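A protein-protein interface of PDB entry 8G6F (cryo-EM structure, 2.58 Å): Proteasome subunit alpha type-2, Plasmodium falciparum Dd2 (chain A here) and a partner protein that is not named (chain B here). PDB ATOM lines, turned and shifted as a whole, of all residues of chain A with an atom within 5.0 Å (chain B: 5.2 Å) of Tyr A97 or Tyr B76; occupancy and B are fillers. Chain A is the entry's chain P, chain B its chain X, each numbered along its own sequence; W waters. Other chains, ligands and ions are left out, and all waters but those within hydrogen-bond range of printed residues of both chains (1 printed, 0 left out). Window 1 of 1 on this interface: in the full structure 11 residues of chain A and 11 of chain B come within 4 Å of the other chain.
The side-chain hydroxyl (OH) of Tyr A101 lies within hydrogen-bond range of the guanidinium group (NH2) of Arg B72. The side-chain hydroxyl of Tyr B76 sits at hydrogen-bond distance from the side-chain hydroxyl of Tyr A97, at 2.7 Å. NE of Arg B79 is in salt-bridge range of OE2 of Glu A109 (3.2 Å). The side-chain sulfur of Cys B88 lies within hydrogen-bond range of the side-chain hydroxyl of Ser A103, at 3.1 Å.
The side-chain carboxylate of Glu B77 sits at hydrogen-bond distance from the backbone NH of Met B84, 3.1 Å away. The side-chain hydroxyl (OG) of Ser A98 sits at hydrogen-bond distance from the backbone carbonyl oxygen (O) of Ser A103, 3.3 Å away.
Gln A100 touches Arg B72. Tyr A101 touches Tyr B76 (OH to CD2, 3.6 Å). CE of Met B84 touches CE1 of Tyr A101, at 3.3 Å. CA of Cys B88 touches O of Tyr A101, at 3.7 Å. OH of Tyr B76 touches CD1 of Leu A106 (3.5 Å). Leu A106 touches Gln B80. Glu A109 touches Gln B80.
Of chain B, only Tyr B76 (2.7 Å) comes within 4 Å of Tyr A97. Of chain A, only Tyr A97 (2.7 Å), Tyr A101 (3.6 Å) and Leu A106 (3.5 Å) come within 4 Å of Tyr B76. Of the printed residues of chain A, Arg B72 touches Gln A100 and Tyr A101. Of the printed residues of chain A, Gln B80 touches Leu A106 and Glu A109. Of the printed residues of chain B, Tyr A101 touches Arg B72 (3.5 Å), Tyr B76 (3.6 Å), Met B84 (3.3 Å) and Cys B88 (3.7 Å). Of the printed residues of chain A, Arg B79 touches Glu A109 (3.2 Å). Printed residues of chain B within 4 Å of Gln A100: Arg B72. Ser A98 touches none of the printed residues of chain B. Ile A105 touches none of the printed residues of chain B. The nearest residue of chain B that does not touch Tyr A97 is Cys B88 (4.6 Å). The nearest printed residue of chain A that does not touch Tyr B76 is Ser A103 (6.0 Å). The nearest printed residue of chain B that does not touch Gln A100 is Cys B88 (4.9 Å).
Hydrophobic or aromatic side chains of chain A within 4 Å of the printed part of chain B: Tyr A97, Tyr A101 and Leu A106. Of the 15 printed residues of chain B, 6 touch a printed residue of chain A. Printed residues of chain B that touch a printed residue of chain A: Arg B72, Tyr B76, Arg B79, Gln B80, Met B84 and Cys B88. Among the printed residues, 11 pairs touch across the chains.
Water W1 bridges NE of Arg B72 (3.0 Å) and OH of Tyr A101 (3.1 Å).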
ATOM      1  N   GLU A  93       8.677  -8.061  40.531  1.00  0.00           N
ATOM      2  CA  GLU A  93       8.014  -8.195  39.237  1.00  0.00           C
ATOM      3  C   GLU A  93       7.487  -6.854  38.745  1.00  0.00           C
ATOM      4  O   GLU A  93       7.573  -6.543  37.550  1.00  0.00           O
ATOM      5  CB  GLU A  93       6.872  -9.205  39.334  1.00  0.00           C
ATOM      6  CG  GLU A  93       7.317 -10.644  39.493  1.00  0.00           C
ATOM      7  CD  GLU A  93       8.345 -11.061  38.462  1.00  0.00           C
ATOM      8  OE1 GLU A  93       8.126 -10.794  37.263  1.00  0.00           O
ATOM      9  OE2 GLU A  93       9.371 -11.656  38.851  1.00  0.00           O
ATOM     10  N   ALA A  94       6.921  -6.055  39.647  1.00  0.00           N
ATOM     11  CA  ALA A  94       6.412  -4.748  39.253  1.00  0.00           C
ATOM     12  C   ALA A  94       7.530  -3.856  38.732  1.00  0.00           C
ATOM     13  O   ALA A  94       7.377  -3.200  37.695  1.00  0.00           O
ATOM     14  CB  ALA A  94       5.700  -4.087  40.432  1.00  0.00           C
ATOM     15  N   ILE A  95       8.672  -3.825  39.426  1.00  0.00           N
ATOM     16  CA  ILE A  95       9.740  -2.954  38.944  1.00  0.00           C
ATOM     17  C   ILE A  95      10.373  -3.528  37.682  1.00  0.00           C
ATOM     18  O   ILE A  95      10.902  -2.779  36.859  1.00  0.00           O
ATOM     19  CB  ILE A  95      10.797  -2.672  40.031  1.00  0.00           C
ATOM     20  CG1 ILE A  95      11.688  -3.888  40.274  1.00  0.00           C
ATOM     21  CG2 ILE A  95      10.142  -2.196  41.313  1.00  0.00           C
ATOM     22  CD1 ILE A  95      13.055  -3.750  39.655  1.00  0.00           C
ATOM     23  N   ARG A  96      10.328  -4.848  37.490  1.00  0.00           N
ATOM     24  CA  ARG A  96      10.785  -5.421  36.226  1.00  0.00           C
ATOM     25  C   ARG A  96       9.918  -4.943  35.069  1.00  0.00           C
ATOM     26  O   ARG A  96      10.423  -4.514  34.021  1.00  0.00           O
ATOM     27  CB  ARG A  96      10.769  -6.943  36.310  1.00  0.00           C
ATOM     28  CG  ARG A  96      11.742  -7.621  35.377  1.00  0.00           C
ATOM     29  CD  ARG A  96      11.491  -9.120  35.297  1.00  0.00           C
ATOM     30  NE  ARG A  96      11.586  -9.769  36.599  1.00  0.00           N
ATOM     31  CZ  ARG A  96      12.709  -9.907  37.292  1.00  0.00           C
ATOM     32  NH1 ARG A  96      13.864  -9.453  36.836  1.00  0.00           N
ATOM     33  NH2 ARG A  96      12.671 -10.518  38.471  1.00  0.00           N
ATOM     34  N   TYR A  97       8.600  -4.999  35.247  1.00  0.00           N
ATOM     35  CA  TYR A  97       7.705  -4.494  34.216  1.00  0.00           C
ATOM     36  C   TYR A  97       7.949  -3.014  33.963  1.00  0.00           C
ATOM     37  O   TYR A  97       7.913  -2.560  32.816  1.00  0.00           O
ATOM     38  CB  TYR A  97       6.254  -4.740  34.623  1.00  0.00           C
ATOM     39  CG  TYR A  97       5.232  -4.315  33.596  1.00  0.00           C
ATOM     40  CD1 TYR A  97       4.935  -2.978  33.396  1.00  0.00           C
ATOM     41  CD2 TYR A  97       4.551  -5.253  32.840  1.00  0.00           C
ATOM     42  CE1 TYR A  97       4.004  -2.587  32.470  1.00  0.00           C
ATOM     43  CE2 TYR A  97       3.613  -4.870  31.910  1.00  0.00           C
ATOM     44  CZ  TYR A  97       3.345  -3.533  31.731  1.00  0.00           C
ATOM     45  OH  TYR A  97       2.414  -3.136  30.806  1.00  0.00           O
ATOM     46  N   SER A  98       8.162  -2.238  35.025  1.00  0.00           N
ATOM     47  CA  SER A  98       8.421  -0.813  34.847  1.00  0.00           C
ATOM     48  C   SER A  98       9.714  -0.580  34.080  1.00  0.00           C
ATOM     49  O   SER A  98       9.765   0.261  33.180  1.00  0.00           O
ATOM     50  CB  SER A  98       8.471  -0.115  36.203  1.00  0.00           C
ATOM     51  OG  SER A  98       7.173   0.044  36.737  1.00  0.00           O
ATOM     52  N   LEU A  99      10.770  -1.322  34.413  1.00  0.00           N
ATOM     53  CA  LEU A  99      12.025  -1.190  33.686  1.00  0.00           C
ATOM     54  C   LEU A  99      11.852  -1.530  32.217  1.00  0.00           C
ATOM     55  O   LEU A  99      12.539  -0.962  31.362  1.00  0.00           O
ATOM     56  CB  LEU A  99      13.087  -2.095  34.303  1.00  0.00           C
ATOM     57  CG  LEU A  99      13.976  -1.477  35.374  1.00  0.00           C
ATOM     58  CD1 LEU A  99      14.848  -2.541  36.002  1.00  0.00           C
ATOM     59  CD2 LEU A  99      14.819  -0.373  34.787  1.00  0.00           C
ATOM     60  N   GLN A 100      10.959  -2.464  31.905  1.00  0.00           N
ATOM     61  CA  GLN A 100      10.784  -2.865  30.515  1.00  0.00           C
ATOM     62  C   GLN A 100       9.928  -1.871  29.735  1.00  0.00           C
ATOM     63  O   GLN A 100      10.289  -1.473  28.625  1.00  0.00           O
ATOM     64  CB  GLN A 100      10.161  -4.256  30.459  1.00  0.00           C
ATOM     65  CG  GLN A 100      10.538  -5.043  29.240  1.00  0.00           C
ATOM     66  CD  GLN A 100      11.495  -6.159  29.560  1.00  0.00           C
ATOM     67  OE1 GLN A 100      11.119  -7.151  30.181  1.00  0.00           O
ATOM     68  NE2 GLN A 100      12.746  -6.005  29.144  1.00  0.00           N
ATOM     69  N   TYR A 101       8.794  -1.457  30.297  1.00  0.00           N
ATOM     70  CA  TYR A 101       7.763  -0.756  29.541  1.00  0.00           C
ATOM     71  C   TYR A 101       7.573   0.696  29.950  1.00  0.00           C
ATOM     72  O   TYR A 101       6.654   1.345  29.444  1.00  0.00           O
ATOM     73  CB  TYR A 101       6.429  -1.494  29.679  1.00  0.00           C
ATOM     74  CG  TYR A 101       6.469  -2.895  29.129  1.00  0.00           C
ATOM     75  CD1 TYR A 101       6.505  -3.119  27.765  1.00  0.00           C
ATOM     76  CD2 TYR A 101       6.484  -3.994  29.973  1.00  0.00           C
ATOM     77  CE1 TYR A 101       6.549  -4.391  27.258  1.00  0.00           C
ATOM     78  CE2 TYR A 101       6.527  -5.270  29.475  1.00  0.00           C
ATOM     79  CZ  TYR A 101       6.560  -5.464  28.114  1.00  0.00           C
ATOM     80  OH  TYR A 101       6.603  -6.734  27.600  1.00  0.00           O
ATOM     81  N   GLY A 102       8.396   1.225  30.850  1.00  0.00           N
ATOM     82  CA  GLY A 102       8.325   2.618  31.225  1.00  0.00           C
ATOM     83  C   GLY A 102       7.117   3.027  32.035  1.00  0.00           C
ATOM     84  O   GLY A 102       7.123   4.125  32.599  1.00  0.00           O
ATOM     85  N   SER A 103       6.085   2.199  32.122  1.00  0.00           N
ATOM     86  CA  SER A 103       4.882   2.530  32.869  1.00  0.00           C
ATOM     87  C   SER A 103       4.661   1.500  33.967  1.00  0.00           C
ATOM     88  O   SER A 103       5.340   0.473  34.039  1.00  0.00           O
ATOM     89  CB  SER A 103       3.658   2.602  31.949  1.00  0.00           C
ATOM     90  OG  SER A 103       3.468   1.391  31.248  1.00  0.00           O
ATOM     91  N   GLU A 104       3.697   1.794  34.831  1.00  0.00           N
ATOM     92  CA  GLU A 104       3.406   0.924  35.958  1.00  0.00           C
ATOM     93  C   GLU A 104       2.746  -0.370  35.498  1.00  0.00           C
ATOM     94  O   GLU A 104       1.985  -0.396  34.528  1.00  0.00           O
ATOM     95  CB  GLU A 104       2.501   1.636  36.952  1.00  0.00           C
ATOM     96  CG  GLU A 104       2.694   1.162  38.363  1.00  0.00           C
ATOM     97  CD  GLU A 104       1.419   1.188  39.152  1.00  0.00           C
ATOM     98  OE1 GLU A 104       0.671   2.177  39.039  1.00  0.00           O
ATOM     99  OE2 GLU A 104       1.162   0.216  39.889  1.00  0.00           O
ATOM    100  N   ILE A 105       3.035  -1.454  36.222  1.00  0.00           N
ATOM    101  CA  ILE A 105       2.520  -2.761  35.840  1.00  0.00           C
ATOM    102  C   ILE A 105       1.001  -2.770  35.919  1.00  0.00           C
ATOM    103  O   ILE A 105       0.388  -2.082  36.742  1.00  0.00           O
ATOM    104  CB  ILE A 105       3.114  -3.872  36.723  1.00  0.00           C
ATOM    105  CG1 ILE A 105       2.693  -5.245  36.199  1.00  0.00           C
ATOM    106  CG2 ILE A 105       2.674  -3.711  38.169  1.00  0.00           C
ATOM    107  CD1 ILE A 105       3.611  -6.356  36.604  1.00  0.00           C
ATOM    108  N   LEU A 106       0.387  -3.567  35.053  1.00  0.00           N
ATOM    109  CA  LEU A 106      -1.056  -3.729  35.065  1.00  0.00           C
ATOM    110  C   LEU A 106      -1.452  -4.798  36.074  1.00  0.00           C
ATOM    111  O   LEU A 106      -0.742  -5.790  36.263  1.00  0.00           O
ATOM    112  CB  LEU A 106      -1.556  -4.090  33.669  1.00  0.00           C
ATOM    113  CG  LEU A 106      -1.257  -3.017  32.619  1.00  0.00           C
ATOM    114  CD1 LEU A 106      -0.994  -3.630  31.261  1.00  0.00           C
ATOM    115  CD2 LEU A 106      -2.398  -2.026  32.538  1.00  0.00           C
ATOM    116  N   GLU A 109      -1.728  -8.342  34.788  1.00  0.00           N
ATOM    117  CA  GLU A 109      -0.423  -8.926  34.500  1.00  0.00           C
ATOM    118  C   GLU A 109       0.282  -9.359  35.782  1.00  0.00           C
ATOM    119  O   GLU A 109       0.836 -10.465  35.866  1.00  0.00           O
ATOM    120  CB  GLU A 109       0.419  -7.912  33.725  1.00  0.00           C
ATOM    121  CG  GLU A 109       1.792  -8.397  33.306  1.00  0.00           C
ATOM    122  CD  GLU A 109       1.730  -9.476  32.250  1.00  0.00           C
ATOM    123  OE1 GLU A 109       0.610  -9.865  31.856  1.00  0.00           O
ATOM    124  OE2 GLU A 109       2.803  -9.935  31.809  1.00  0.00           O
ATOM    125  N   TYR B  71       7.439 -10.560  17.927  1.00  0.00           N
ATOM    126  CA  TYR B  71       7.307 -11.573  18.967  1.00  0.00           C
ATOM    127  C   TYR B  71       6.863 -10.950  20.284  1.00  0.00           C
ATOM    128  O   TYR B  71       5.880 -11.385  20.900  1.00  0.00           O
ATOM    129  CB  TYR B  71       8.647 -12.293  19.115  1.00  0.00           C
ATOM    130  CG  TYR B  71       8.759 -13.271  20.253  1.00  0.00           C
ATOM    131  CD1 TYR B  71       9.101 -12.850  21.526  1.00  0.00           C
ATOM    132  CD2 TYR B  71       8.567 -14.622  20.044  1.00  0.00           C
ATOM    133  CE1 TYR B  71       9.218 -13.745  22.559  1.00  0.00           C
ATOM    134  CE2 TYR B  71       8.681 -15.522  21.069  1.00  0.00           C
ATOM    135  CZ  TYR B  71       9.008 -15.081  22.323  1.00  0.00           C
ATOM    136  OH  TYR B  71       9.124 -15.986  23.348  1.00  0.00           O
ATOM    137  N   ARG B  72       7.571  -9.908  20.719  1.00  0.00           N
ATOM    138  CA  ARG B  72       7.272  -9.281  22.001  1.00  0.00           C
ATOM    139  C   ARG B  72       5.879  -8.670  22.009  1.00  0.00           C
ATOM    140  O   ARG B  72       5.123  -8.835  22.973  1.00  0.00           O
ATOM    141  CB  ARG B  72       8.322  -8.217  22.310  1.00  0.00           C
ATOM    142  CG  ARG B  72       9.717  -8.767  22.523  1.00  0.00           C
ATOM    143  CD  ARG B  72       9.847  -9.452  23.864  1.00  0.00           C
ATOM    144  NE  ARG B  72       9.499  -8.566  24.968  1.00  0.00           N
ATOM    145  CZ  ARG B  72      10.367  -7.839  25.657  1.00  0.00           C
ATOM    146  NH1 ARG B  72      11.661  -7.865  25.388  1.00  0.00           N
ATOM    147  NH2 ARG B  72       9.924  -7.064  26.641  1.00  0.00           N
ATOM    148  N   VAL B  73       5.522  -7.951  20.946  1.00  0.00           N
ATOM    149  CA  VAL B  73       4.225  -7.286  20.900  1.00  0.00           C
ATOM    150  C   VAL B  73       3.104  -8.313  20.887  1.00  0.00           C
ATOM    151  O   VAL B  73       2.088  -8.146  21.567  1.00  0.00           O
ATOM    152  CB  VAL B  73       4.149  -6.347  19.682  1.00  0.00           C
ATOM    153  CG1 VAL B  73       2.720  -5.929  19.413  1.00  0.00           C
ATOM    154  CG2 VAL B  73       5.014  -5.130  19.904  1.00  0.00           C
ATOM    155  N   ASN B  74       3.259  -9.382  20.105  1.00  0.00           N
ATOM    156  CA  ASN B  74       2.221 -10.400  20.045  1.00  0.00           C
ATOM    157  C   ASN B  74       2.034 -11.073  21.393  1.00  0.00           C
ATOM    158  O   ASN B  74       0.900 -11.304  21.825  1.00  0.00           O
ATOM    159  CB  ASN B  74       2.567 -11.432  18.976  1.00  0.00           C
ATOM    160  CG  ASN B  74       2.250 -10.952  17.582  1.00  0.00           C
ATOM    161  OD1 ASN B  74       1.730  -9.856  17.395  1.00  0.00           O
ATOM    162  ND2 ASN B  74       2.564 -11.769  16.591  1.00  0.00           N
ATOM    163  N   LEU B  75       3.130 -11.398  22.078  1.00  0.00           N
ATOM    164  CA  LEU B  75       3.004 -12.016  23.393  1.00  0.00           C
ATOM    165  C   LEU B  75       2.328 -11.074  24.378  1.00  0.00           C
ATOM    166  O   LEU B  75       1.415 -11.469  25.113  1.00  0.00           O
ATOM    167  CB  LEU B  75       4.376 -12.435  23.909  1.00  0.00           C
ATOM    168  CG  LEU B  75       4.671 -13.919  23.723  1.00  0.00           C
ATOM    169  CD1 LEU B  75       6.160 -14.149  23.729  1.00  0.00           C
ATOM    170  CD2 LEU B  75       3.990 -14.737  24.806  1.00  0.00           C
ATOM    171  N   TYR B  76       2.760  -9.814  24.402  1.00  0.00           N
ATOM    172  CA  TYR B  76       2.157  -8.844  25.306  1.00  0.00           C
ATOM    173  C   TYR B  76       0.664  -8.721  25.046  1.00  0.00           C
ATOM    174  O   TYR B  76      -0.145  -8.723  25.979  1.00  0.00           O
ATOM    175  CB  TYR B  76       2.860  -7.496  25.136  1.00  0.00           C
ATOM    176  CG  TYR B  76       2.369  -6.387  26.033  1.00  0.00           C
ATOM    177  CD1 TYR B  76       1.161  -5.752  25.790  1.00  0.00           C
ATOM    178  CD2 TYR B  76       3.128  -5.954  27.107  1.00  0.00           C
ATOM    179  CE1 TYR B  76       0.715  -4.738  26.599  1.00  0.00           C
ATOM    180  CE2 TYR B  76       2.692  -4.938  27.921  1.00  0.00           C
ATOM    181  CZ  TYR B  76       1.488  -4.331  27.663  1.00  0.00           C
ATOM    182  OH  TYR B  76       1.049  -3.315  28.474  1.00  0.00           O
ATOM    183  N   GLU B  77       0.279  -8.624  23.774  1.00  0.00           N
ATOM    184  CA  GLU B  77      -1.116  -8.375  23.440  1.00  0.00           C
ATOM    185  C   GLU B  77      -1.982  -9.596  23.712  1.00  0.00           C
ATOM    186  O   GLU B  77      -3.120  -9.457  24.169  1.00  0.00           O
ATOM    187  CB  GLU B  77      -1.228  -7.939  21.982  1.00  0.00           C
ATOM    188  CG  GLU B  77      -0.628  -6.572  21.727  1.00  0.00           C
ATOM    189  CD  GLU B  77      -0.787  -6.106  20.295  1.00  0.00           C
ATOM    190  OE1 GLU B  77      -0.721  -6.947  19.378  1.00  0.00           O
ATOM    191  OE2 GLU B  77      -0.966  -4.892  20.085  1.00  0.00           O
ATOM    192  N   VAL B  78      -1.473 -10.800  23.448  1.00  0.00           N
ATOM    193  CA  VAL B  78      -2.262 -11.990  23.742  1.00  0.00           C
ATOM    194  C   VAL B  78      -2.419 -12.164  25.246  1.00  0.00           C
ATOM    195  O   VAL B  78      -3.476 -12.586  25.724  1.00  0.00           O
ATOM    196  CB  VAL B  78      -1.641 -13.236  23.081  1.00  0.00           C
ATOM    197  CG1 VAL B  78      -0.473 -13.765  23.889  1.00  0.00           C
ATOM    198  CG2 VAL B  78      -2.695 -14.317  22.900  1.00  0.00           C
ATOM    199  N   ARG B  79      -1.380 -11.837  26.017  1.00  0.00           N
ATOM    200  CA  ARG B  79      -1.476 -11.972  27.467  1.00  0.00           C
ATOM    201  C   ARG B  79      -2.451 -10.959  28.054  1.00  0.00           C
ATOM    202  O   ARG B  79      -3.285 -11.304  28.896  1.00  0.00           O
ATOM    203  CB  ARG B  79      -0.094 -11.813  28.095  1.00  0.00           C
ATOM    204  CG  ARG B  79       0.739 -13.079  28.073  1.00  0.00           C
ATOM    205  CD  ARG B  79       2.075 -12.885  28.760  1.00  0.00           C
ATOM    206  NE  ARG B  79       1.923 -12.539  30.168  1.00  0.00           N
ATOM    207  CZ  ARG B  79       1.958 -13.405  31.173  1.00  0.00           C
ATOM    208  NH1 ARG B  79       2.138 -14.699  30.969  1.00  0.00           N
ATOM    209  NH2 ARG B  79       1.806 -12.962  32.416  1.00  0.00           N
ATOM    210  N   GLN B  80      -2.364  -9.701  27.623  1.00  0.00           N
ATOM    211  CA  GLN B  80      -3.173  -8.641  28.209  1.00  0.00           C
ATOM    212  C   GLN B  80      -4.564  -8.533  27.603  1.00  0.00           C
ATOM    213  O   GLN B  80      -5.417  -7.856  28.182  1.00  0.00           O
ATOM    214  CB  GLN B  80      -2.456  -7.299  28.056  1.00  0.00           C
ATOM    215  CG  GLN B  80      -2.871  -6.256  29.072  1.00  0.00           C
ATOM    216  CD  GLN B  80      -2.404  -6.597  30.471  1.00  0.00           C
ATOM    217  OE1 GLN B  80      -1.303  -7.115  30.656  1.00  0.00           O
ATOM    218  NE2 GLN B  80      -3.240  -6.311  31.463  1.00  0.00           N
ATOM    219  N   ASP B  81      -4.819  -9.179  26.470  1.00  0.00           N
ATOM    220  CA  ASP B  81      -6.099  -9.058  25.779  1.00  0.00           C
ATOM    221  C   ASP B  81      -6.381  -7.606  25.403  1.00  0.00           C
ATOM    222  O   ASP B  81      -7.526  -7.151  25.418  1.00  0.00           O
ATOM    223  CB  ASP B  81      -7.236  -9.629  26.624  1.00  0.00           C
ATOM    224  CG  ASP B  81      -8.488  -9.878  25.817  1.00  0.00           C
ATOM    225  OD1 ASP B  81      -8.533  -9.447  24.647  1.00  0.00           O
ATOM    226  OD2 ASP B  81      -9.428 -10.504  26.351  1.00  0.00           O
ATOM    227  N   ALA B  82      -5.327  -6.872  25.061  1.00  0.00           N
ATOM    228  CA  ALA B  82      -5.458  -5.470  24.697  1.00  0.00           C
ATOM    229  C   ALA B  82      -4.320  -5.089  23.765  1.00  0.00           C
ATOM    230  O   ALA B  82      -3.253  -5.706  23.772  1.00  0.00           O
ATOM    231  CB  ALA B  82      -5.453  -4.567  25.933  1.00  0.00           C
ATOM    232  N   GLU B  83      -4.560  -4.057  22.963  1.00  0.00           N
ATOM    233  CA  GLU B  83      -3.520  -3.540  22.087  1.00  0.00           C
ATOM    234  C   GLU B  83      -2.449  -2.836  22.905  1.00  0.00           C
ATOM    235  O   GLU B  83      -2.740  -2.178  23.905  1.00  0.00           O
ATOM    236  CB  GLU B  83      -4.114  -2.576  21.065  1.00  0.00           C
ATOM    237  CG  GLU B  83      -4.597  -3.246  19.794  1.00  0.00           C
ATOM    238  CD  GLU B  83      -4.537  -2.333  18.586  1.00  0.00           C
ATOM    239  OE1 GLU B  83      -4.129  -1.162  18.735  1.00  0.00           O
ATOM    240  OE2 GLU B  83      -4.900  -2.790  17.483  1.00  0.00           O
ATOM    241  N   MET B  84      -1.200  -2.978  22.475  1.00  0.00           N
ATOM    242  CA  MET B  84      -0.093  -2.378  23.202  1.00  0.00           C
ATOM    243  C   MET B  84      -0.085  -0.868  23.015  1.00  0.00           C
ATOM    244  O   MET B  84      -0.295  -0.359  21.911  1.00  0.00           O
ATOM    245  CB  MET B  84       1.231  -2.969  22.729  1.00  0.00           C
ATOM    246  CG  MET B  84       2.422  -2.563  23.568  1.00  0.00           C
ATOM    247  SD  MET B  84       3.900  -3.487  23.145  1.00  0.00           S
ATOM    248  CE  MET B  84       4.763  -3.442  24.701  1.00  0.00           C
ATOM    249  N   CYS B  88       4.369   2.401  25.723  1.00  0.00           N
ATOM    250  CA  CYS B  88       4.910   1.141  26.211  1.00  0.00           C
ATOM    251  C   CYS B  88       5.783   0.482  25.156  1.00  0.00           C
ATOM    252  O   CYS B  88       6.865  -0.027  25.466  1.00  0.00           O
ATOM    253  CB  CYS B  88       3.773   0.211  26.628  1.00  0.00           C
ATOM    254  SG  CYS B  88       3.072   0.603  28.240  1.00  0.00           S
HETATM  255  O   HOH W   1       6.603  -9.107  25.581  1.00  0.00           O
